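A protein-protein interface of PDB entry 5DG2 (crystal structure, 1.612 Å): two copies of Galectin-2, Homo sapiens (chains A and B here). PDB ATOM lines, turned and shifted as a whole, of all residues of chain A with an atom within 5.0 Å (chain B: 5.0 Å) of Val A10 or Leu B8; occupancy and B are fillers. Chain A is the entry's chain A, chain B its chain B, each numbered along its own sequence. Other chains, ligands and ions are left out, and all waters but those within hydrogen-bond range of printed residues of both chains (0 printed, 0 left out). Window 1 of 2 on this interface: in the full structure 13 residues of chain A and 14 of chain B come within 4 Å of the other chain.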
ATOM      1  N   LEU A   8      -9.140 -22.876 -12.332  1.00  0.00           N
ATOM      2  CA  LEU A   8      -9.755 -22.572 -11.049  1.00  0.00           C
ATOM      3  C   LEU A   8     -10.016 -23.800 -10.166  1.00  0.00           C
ATOM      4  O   LEU A   8     -10.649 -24.764 -10.589  1.00  0.00           O
ATOM      5  CB  LEU A   8     -11.047 -21.814 -11.290  1.00  0.00           C
ATOM      6  CG  LEU A   8     -11.616 -21.119 -10.065  1.00  0.00           C
ATOM      7  CD1 LEU A   8     -12.043 -19.702 -10.426  1.00  0.00           C
ATOM      8  CD2 LEU A   8     -12.782 -21.909  -9.519  1.00  0.00           C
ATOM      9  N   GLU A   9      -9.500 -23.761  -8.941  1.00  0.00           N
ATOM     10  CA  GLU A   9      -9.816 -24.749  -7.907  1.00  0.00           C
ATOM     11  C   GLU A   9     -10.498 -24.077  -6.725  1.00  0.00           C
ATOM     12  O   GLU A   9     -10.065 -23.010  -6.273  1.00  0.00           O
ATOM     13  CB  GLU A   9      -8.556 -25.459  -7.408  1.00  0.00           C
ATOM     14  CG  GLU A   9      -8.097 -26.646  -8.232  1.00  0.00           C
ATOM     15  CD  GLU A   9      -7.142 -27.543  -7.454  1.00  0.00           C
ATOM     16  OE1 GLU A   9      -6.578 -27.074  -6.440  1.00  0.00           O
ATOM     17  OE2 GLU A   9      -6.972 -28.721  -7.847  1.00  0.00           O
ATOM     18  N   VAL A  10     -11.551 -24.699  -6.214  1.00  0.00           N
ATOM     19  CA  VAL A  10     -12.160 -24.244  -4.973  1.00  0.00           C
ATOM     20  C   VAL A  10     -12.065 -25.368  -3.947  1.00  0.00           C
ATOM     21  O   VAL A  10     -12.421 -26.503  -4.236  1.00  0.00           O
ATOM     22  CB  VAL A  10     -13.632 -23.834  -5.171  1.00  0.00           C
ATOM     23  CG1 VAL A  10     -14.240 -23.335  -3.850  1.00  0.00           C
ATOM     24  CG2 VAL A  10     -13.752 -22.773  -6.247  1.00  0.00           C
ATOM     25  N   LYS A  11     -11.575 -25.061  -2.751  1.00  0.00           N
ATOM     26  CA  LYS A  11     -11.440 -26.076  -1.715  1.00  0.00           C
ATOM     27  C   LYS A  11     -12.161 -25.687  -0.429  1.00  0.00           C
ATOM     28  O   LYS A  11     -12.469 -24.509  -0.206  1.00  0.00           O
ATOM     29  CB  LYS A  11      -9.965 -26.341  -1.408  1.00  0.00           C
ATOM     30  CG  LYS A  11      -9.175 -27.014  -2.504  1.00  0.00           C
ATOM     31  CD  LYS A  11      -7.802 -27.420  -1.992  1.00  0.00           C
ATOM     32  CE  LYS A  11      -7.064 -28.275  -3.005  1.00  0.00           C
ATOM     33  NZ  LYS A  11      -5.760 -28.752  -2.467  1.00  0.00           N
ATOM     34  N   ASN A  12     -12.427 -26.689   0.403  1.00  0.00           N
ATOM     35  CA  ASN A  12     -13.121 -26.509   1.683  1.00  0.00           C
ATOM     36  C   ASN A  12     -14.553 -26.018   1.525  1.00  0.00           C
ATOM     37  O   ASN A  12     -15.084 -25.322   2.396  1.00  0.00           O
ATOM     38  CB  ASN A  12     -12.366 -25.532   2.594  1.00  0.00           C
ATOM     39  CG  ASN A  12     -10.926 -25.933   2.824  1.00  0.00           C
ATOM     40  OD1 ASN A  12     -10.603 -27.120   2.910  1.00  0.00           O
ATOM     41  ND2 ASN A  12     -10.048 -24.939   2.939  1.00  0.00           N
ATOM     42  N   MET A  13     -15.176 -26.362   0.405  1.00  0.00           N
ATOM     43  CA  MET A  13     -16.612 -26.193   0.269  1.00  0.00           C
ATOM     44  C   MET A  13     -17.348 -27.107   1.230  1.00  0.00           C
ATOM     45  O   MET A  13     -16.774 -28.054   1.778  1.00  0.00           O
ATOM     46  CB  MET A  13     -17.064 -26.514  -1.150  1.00  0.00           C
ATOM     47  CG  MET A  13     -16.679 -25.512  -2.191  1.00  0.00           C
ATOM     48  SD  MET A  13     -17.568 -25.939  -3.712  1.00  0.00           S
ATOM     49  CE  MET A  13     -17.228 -27.701  -3.903  1.00  0.00           C
ATOM     50  N   SER A 118     -16.296 -31.059  -1.108  1.00  0.00           N
ATOM     51  CA  SER A 118     -15.495 -29.934  -0.635  1.00  0.00           C
ATOM     52  C   SER A 118     -14.661 -29.319  -1.737  1.00  0.00           C
ATOM     53  O   SER A 118     -14.082 -28.246  -1.563  1.00  0.00           O
ATOM     54  CB  SER A 118     -14.571 -30.374   0.496  1.00  0.00           C
ATOM     55  OG  SER A 118     -13.545 -31.221   0.005  1.00  0.00           O
ATOM     56  N   TYR A 119     -14.592 -29.996  -2.876  1.00  0.00           N
ATOM     57  CA  TYR A 119     -13.627 -29.638  -3.900  1.00  0.00           C
ATOM     58  C   TYR A 119     -14.293 -29.432  -5.243  1.00  0.00           C
ATOM     59  O   TYR A 119     -15.087 -30.268  -5.691  1.00  0.00           O
ATOM     60  CB  TYR A 119     -12.546 -30.729  -3.995  1.00  0.00           C
ATOM     61  CG  TYR A 119     -11.544 -30.593  -5.129  1.00  0.00           C
ATOM     62  CD1 TYR A 119     -10.413 -29.786  -5.003  1.00  0.00           C
ATOM     63  CD2 TYR A 119     -11.707 -31.308  -6.313  1.00  0.00           C
ATOM     64  CE1 TYR A 119      -9.487 -29.678  -6.043  1.00  0.00           C
ATOM     65  CE2 TYR A 119     -10.783 -31.204  -7.349  1.00  0.00           C
ATOM     66  CZ  TYR A 119      -9.683 -30.390  -7.206  1.00  0.00           C
ATOM     67  OH  TYR A 119      -8.773 -30.299  -8.244  1.00  0.00           O
ATOM     68  N   LEU A 120     -13.964 -28.313  -5.879  1.00  0.00           N
ATOM     69  CA  LEU A 120     -14.383 -28.032  -7.251  1.00  0.00           C
ATOM     70  C   LEU A 120     -13.179 -27.597  -8.073  1.00  0.00           C
ATOM     71  O   LEU A 120     -12.363 -26.782  -7.624  1.00  0.00           O
ATOM     72  CB  LEU A 120     -15.457 -26.940  -7.278  1.00  0.00           C
ATOM     73  CG  LEU A 120     -15.718 -26.253  -8.618  1.00  0.00           C
ATOM     74  CD1 LEU A 120     -16.512 -27.152  -9.518  1.00  0.00           C
ATOM     75  CD2 LEU A 120     -16.447 -24.942  -8.408  1.00  0.00           C
ATOM     76  N   SER A 121     -13.050 -28.124  -9.288  1.00  0.00           N
ATOM     77  CA  SER A 121     -11.960 -27.687 -10.159  1.00  0.00           C
ATOM     78  C   SER A 121     -12.377 -27.669 -11.621  1.00  0.00           C
ATOM     79  O   SER A 121     -13.015 -28.599 -12.115  1.00  0.00           O
ATOM     80  CB  SER A 121     -10.737 -28.582  -9.987  1.00  0.00           C
ATOM     81  OG  SER A 121     -10.902 -29.799 -10.699  1.00  0.00           O
ATOM     82  N   PHE A 131     -19.673 -18.402  -9.321  1.00  0.00           N
ATOM     83  CA  PHE A 131     -19.850 -19.605  -8.517  1.00  0.00           C
ATOM     84  C   PHE A 131     -20.962 -19.270  -7.521  1.00  0.00           C
ATOM     85  O   PHE A 131     -20.897 -18.223  -6.890  1.00  0.00           O
ATOM     86  CB  PHE A 131     -18.501 -19.940  -7.840  1.00  0.00           C
ATOM     87  CG  PHE A 131     -18.578 -20.879  -6.664  1.00  0.00           C
ATOM     88  CD1 PHE A 131     -18.930 -20.420  -5.402  1.00  0.00           C
ATOM     89  CD2 PHE A 131     -18.196 -22.203  -6.800  1.00  0.00           C
ATOM     90  CE1 PHE A 131     -18.974 -21.281  -4.315  1.00  0.00           C
ATOM     91  CE2 PHE A 131     -18.229 -23.071  -5.715  1.00  0.00           C
ATOM     92  CZ  PHE A 131     -18.620 -22.614  -4.474  1.00  0.00           C
ATOM     93  N   GLY B   6     -15.736 -24.945   5.144  1.00  0.00           N
ATOM     94  CA  GLY B   6     -16.433 -23.692   4.899  1.00  0.00           C
ATOM     95  C   GLY B   6     -15.500 -22.504   4.721  1.00  0.00           C
ATOM     96  O   GLY B   6     -15.884 -21.473   4.161  1.00  0.00           O
ATOM     97  N   GLU B   7     -14.271 -22.638   5.208  1.00  0.00           N
ATOM     98  CA  GLU B   7     -13.254 -21.630   4.979  1.00  0.00           C
ATOM     99  C   GLU B   7     -12.709 -21.819   3.566  1.00  0.00           C
ATOM    100  O   GLU B   7     -11.596 -22.313   3.368  1.00  0.00           O
ATOM    101  CB  GLU B   7     -12.151 -21.724   6.030  1.00  0.00           C
ATOM    102  CG  GLU B   7     -12.656 -21.445   7.443  1.00  0.00           C
ATOM    103  CD  GLU B   7     -11.536 -21.318   8.449  1.00  0.00           C
ATOM    104  OE1 GLU B   7     -10.503 -21.998   8.271  1.00  0.00           O
ATOM    105  OE2 GLU B   7     -11.689 -20.538   9.420  1.00  0.00           O
ATOM    106  N   LEU B   8     -13.521 -21.399   2.597  1.00  0.00           N
ATOM    107  CA  LEU B   8     -13.213 -21.560   1.176  1.00  0.00           C
ATOM    108  C   LEU B   8     -11.841 -21.031   0.795  1.00  0.00           C
ATOM    109  O   LEU B   8     -11.392 -19.988   1.288  1.00  0.00           O
ATOM    110  CB  LEU B   8     -14.266 -20.854   0.315  1.00  0.00           C
ATOM    111  CG  LEU B   8     -15.289 -21.695  -0.443  1.00  0.00           C
ATOM    112  CD1 LEU B   8     -15.953 -22.680   0.493  1.00  0.00           C
ATOM    113  CD2 LEU B   8     -16.331 -20.799  -1.102  1.00  0.00           C
ATOM    114  N   GLU B   9     -11.174 -21.761  -0.091  1.00  0.00           N
ATOM    115  CA  GLU B   9     -10.001 -21.235  -0.767  1.00  0.00           C
ATOM    116  C   GLU B   9     -10.233 -21.338  -2.259  1.00  0.00           C
ATOM    117  O   GLU B   9     -10.644 -22.383  -2.751  1.00  0.00           O
ATOM    118  CB  GLU B   9      -8.736 -21.994  -0.374  1.00  0.00           C
ATOM    119  CG  GLU B   9      -8.426 -21.932   1.106  1.00  0.00           C
ATOM    120  CD  GLU B   9      -7.306 -22.872   1.499  1.00  0.00           C
ATOM    121  OE1 GLU B   9      -6.705 -23.497   0.595  1.00  0.00           O
ATOM    122  OE2 GLU B   9      -7.021 -22.980   2.711  1.00  0.00           O
ATOM    123  N   VAL B  10     -10.011 -20.247  -2.972  1.00  0.00           N
ATOM    124  CA  VAL B  10     -10.101 -20.264  -4.421  1.00  0.00           C
ATOM    125  C   VAL B  10      -8.707 -20.028  -4.993  1.00  0.00           C
ATOM    126  O   VAL B  10      -8.061 -19.045  -4.644  1.00  0.00           O
ATOM    127  CB  VAL B  10     -11.068 -19.187  -4.945  1.00  0.00           C
ATOM    128  CG1 VAL B  10     -11.186 -19.283  -6.464  1.00  0.00           C
ATOM    129  CG2 VAL B  10     -12.430 -19.324  -4.287  1.00  0.00           C
ATOM    130  N   LEU B 120      -7.959 -16.403  -3.393  1.00  0.00           N
ATOM    131  CA  LEU B 120      -9.005 -15.859  -2.531  1.00  0.00           C
ATOM    132  C   LEU B 120      -9.263 -16.844  -1.408  1.00  0.00           C
ATOM    133  O   LEU B 120      -9.430 -18.042  -1.658  1.00  0.00           O
ATOM    134  CB  LEU B 120     -10.295 -15.611  -3.326  1.00  0.00           C
ATOM    135  CG  LEU B 120     -11.595 -15.316  -2.566  1.00  0.00           C
ATOM    136  CD1 LEU B 120     -11.528 -13.963  -1.905  1.00  0.00           C
ATOM    137  CD2 LEU B 120     -12.795 -15.388  -3.510  1.00  0.00           C
ATOM    138  N   SER B 121      -9.293 -16.374  -0.165  1.00  0.00           N
ATOM    139  CA  SER B 121      -9.693 -17.293   0.887  1.00  0.00           C
ATOM    140  C   SER B 121     -10.524 -16.610   1.948  1.00  0.00           C
ATOM    141  O   SER B 121     -10.446 -15.394   2.144  1.00  0.00           O
ATOM    142  CB  SER B 121      -8.483 -17.963   1.530  1.00  0.00           C
ATOM    143  OG  SER B 121      -7.723 -17.045   2.298  1.00  0.00           O
ATOM    144  N   VAL B 122     -11.322 -17.418   2.634  1.00  0.00           N
ATOM    145  CA  VAL B 122     -12.154 -16.941   3.729  1.00  0.00           C
ATOM    146  C   VAL B 122     -11.755 -17.657   5.006  1.00  0.00           C
ATOM    147  O   VAL B 122     -11.388 -18.829   4.977  1.00  0.00           O
ATOM    148  CB  VAL B 122     -13.643 -17.170   3.414  1.00  0.00           C
ATOM    149  CG1 VAL B 122     -14.519 -16.916   4.630  1.00  0.00           C
ATOM    150  CG2 VAL B 122     -14.040 -16.268   2.285  1.00  0.00           C
ATOM    151  N   ARG B 123     -11.786 -16.942   6.123  1.00  0.00           N
ATOM    152  CA  ARG B 123     -11.530 -17.534   7.422  1.00  0.00           C
ATOM    153  C   ARG B 123     -12.563 -16.996   8.405  1.00  0.00           C
ATOM    154  O   ARG B 123     -13.098 -15.898   8.220  1.00  0.00           O
ATOM    155  CB  ARG B 123     -10.119 -17.212   7.926  1.00  0.00           C
ATOM    156  CG  ARG B 123      -8.984 -17.513   6.951  1.00  0.00           C
ATOM    157  CD  ARG B 123      -8.680 -18.994   6.916  1.00  0.00           C
ATOM    158  NE  ARG B 123      -7.555 -19.311   6.038  1.00  0.00           N
ATOM    159  CZ  ARG B 123      -7.672 -19.897   4.849  1.00  0.00           C
ATOM    160  NH1 ARG B 123      -8.870 -20.229   4.380  1.00  0.00           N
ATOM    161  NH2 ARG B 123      -6.585 -20.151   4.129  1.00  0.00           N
ATOM    162  N   MET B 128     -19.217 -18.126   2.547  1.00  0.00           N
ATOM    163  CA  MET B 128     -19.328 -17.498   1.235  1.00  0.00           C
ATOM    164  C   MET B 128     -20.232 -18.339   0.355  1.00  0.00           C
ATOM    165  O   MET B 128     -19.949 -19.508   0.107  1.00  0.00           O
ATOM    166  CB  MET B 128     -17.953 -17.330   0.587  1.00  0.00           C
ATOM    167  CG  MET B 128     -18.002 -16.572  -0.724  1.00  0.00           C
ATOM    168  SD  MET B 128     -16.352 -16.247  -1.398  1.00  0.00           S
ATOM    169  CE  MET B 128     -15.709 -15.000  -0.307  1.00  0.00           C
ATOM    170  N   PHE B 131     -19.485 -15.999  -5.507  1.00  0.00           N
ATOM    171  CA  PHE B 131     -18.576 -14.971  -5.958  1.00  0.00           C
ATOM    172  C   PHE B 131     -18.661 -14.829  -7.462  1.00  0.00           C
ATOM    173  O   PHE B 131     -19.016 -15.762  -8.198  1.00  0.00           O
ATOM    174  CB  PHE B 131     -17.134 -15.218  -5.482  1.00  0.00           C
ATOM    175  CG  PHE B 131     -16.491 -16.452  -6.040  1.00  0.00           C
ATOM    176  CD1 PHE B 131     -16.488 -17.631  -5.311  1.00  0.00           C
ATOM    177  CD2 PHE B 131     -15.842 -16.418  -7.264  1.00  0.00           C
ATOM    178  CE1 PHE B 131     -15.876 -18.774  -5.813  1.00  0.00           C
ATOM    179  CE2 PHE B 131     -15.231 -17.547  -7.774  1.00  0.00           C
ATOM    180  CZ  PHE B 131     -15.250 -18.732  -7.046  1.00  0.00           C
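The side-chain amide nitrogen (ND2) of Asn A12 lies within hydrogen-bond range of the backbone carbonyl oxygen (O) of Glu B7 (3.1 Å).
The backbone carbonyl oxygen (O) of Phe B131 sits at hydrogen-bond distance from the backbone NH (N) of Phe A131 (2.9 Å).
The backbone NH (N) of Lys A11 is in hydrogen-bond range of the backbone carbonyl oxygen (O) of Glu B9, at 2.8 Å.
The backbone carbonyl oxygen (O) of Asn A12 sits at hydrogen-bond distance from the backbone NH (N) of Gly B6 (2.8 Å).
The backbone NH (N) of Met A13 sits at hydrogen-bond distance from the backbone carbonyl oxygen (O) of Ser A118 (2.9 Å).
The backbone NH of Val B10 is in hydrogen-bond range of the backbone carbonyl oxygen of Leu B120.
The backbone carbonyl oxygen (O) of Leu A120 lies within hydrogen-bond range of the backbone NH (N) of Val A10.
The side-chain carboxylate (OE2) of Glu A9 is in hydrogen-bond range of the side-chain hydroxyl (OH) of Tyr A119.
The backbone NH (N) of Val B122 lies within hydrogen-bond range of the backbone carbonyl oxygen (O) of Leu B8, 2.9 Å away.
OE2 of Glu B9 is in salt-bridge range of NH2 of Arg B123 (3.2 Å).
Glu B9 touches Glu A9 (O to O, 3.6 Å).
Glu A9 touches Val B10.
Val A10 touches Leu B8 (CG1 to CG, 3.9 Å).
Glu B9 touches Val A10.
O of Lys A11 touches CA of Leu B8 (3.3 Å).
CD1 of Leu B8 touches O of Asn A12, at 3.4 Å.
Asn A12 touches Glu B9.
CA of Met A13 touches CD1 of Leu B8, at 3.6 Å.
Printed residues of chain B within 4 Å of Glu A9: Glu B9 and Val B10.
Of chain B, only Leu B8 and Glu B9 come within 4 Å of Val A10.
Of the printed residues of chain B, Phe A131 touches Phe B131.
Of the printed residues of chain A, Leu B8 touches Val A10, Lys A11, Asn A12 and Met A13.
Printed residues of chain A within 4 Å of Val B10: Glu A9 (3.3 Å).
The nearest residue of chain B that does not touch Val A10 is Val B10 (4.2 Å).
Glu B9 touches its own counterpart, Glu A9.
Glu A9 touches Val B10, and with the chains exchanged Val A10 touches Glu B9.
Val A10 touches Leu B8, but with the chains exchanged Leu A8 does not touch Val B10 (4.1 Å).
Phe B131 touches its own counterpart, Phe A131.
Positions printed for both chains: 8, 9, 10, 120, 121 and 131.
Of the 12 pairs that touch across the chains among the printed residues, 4 have their exchanged pair printed and touching as well.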
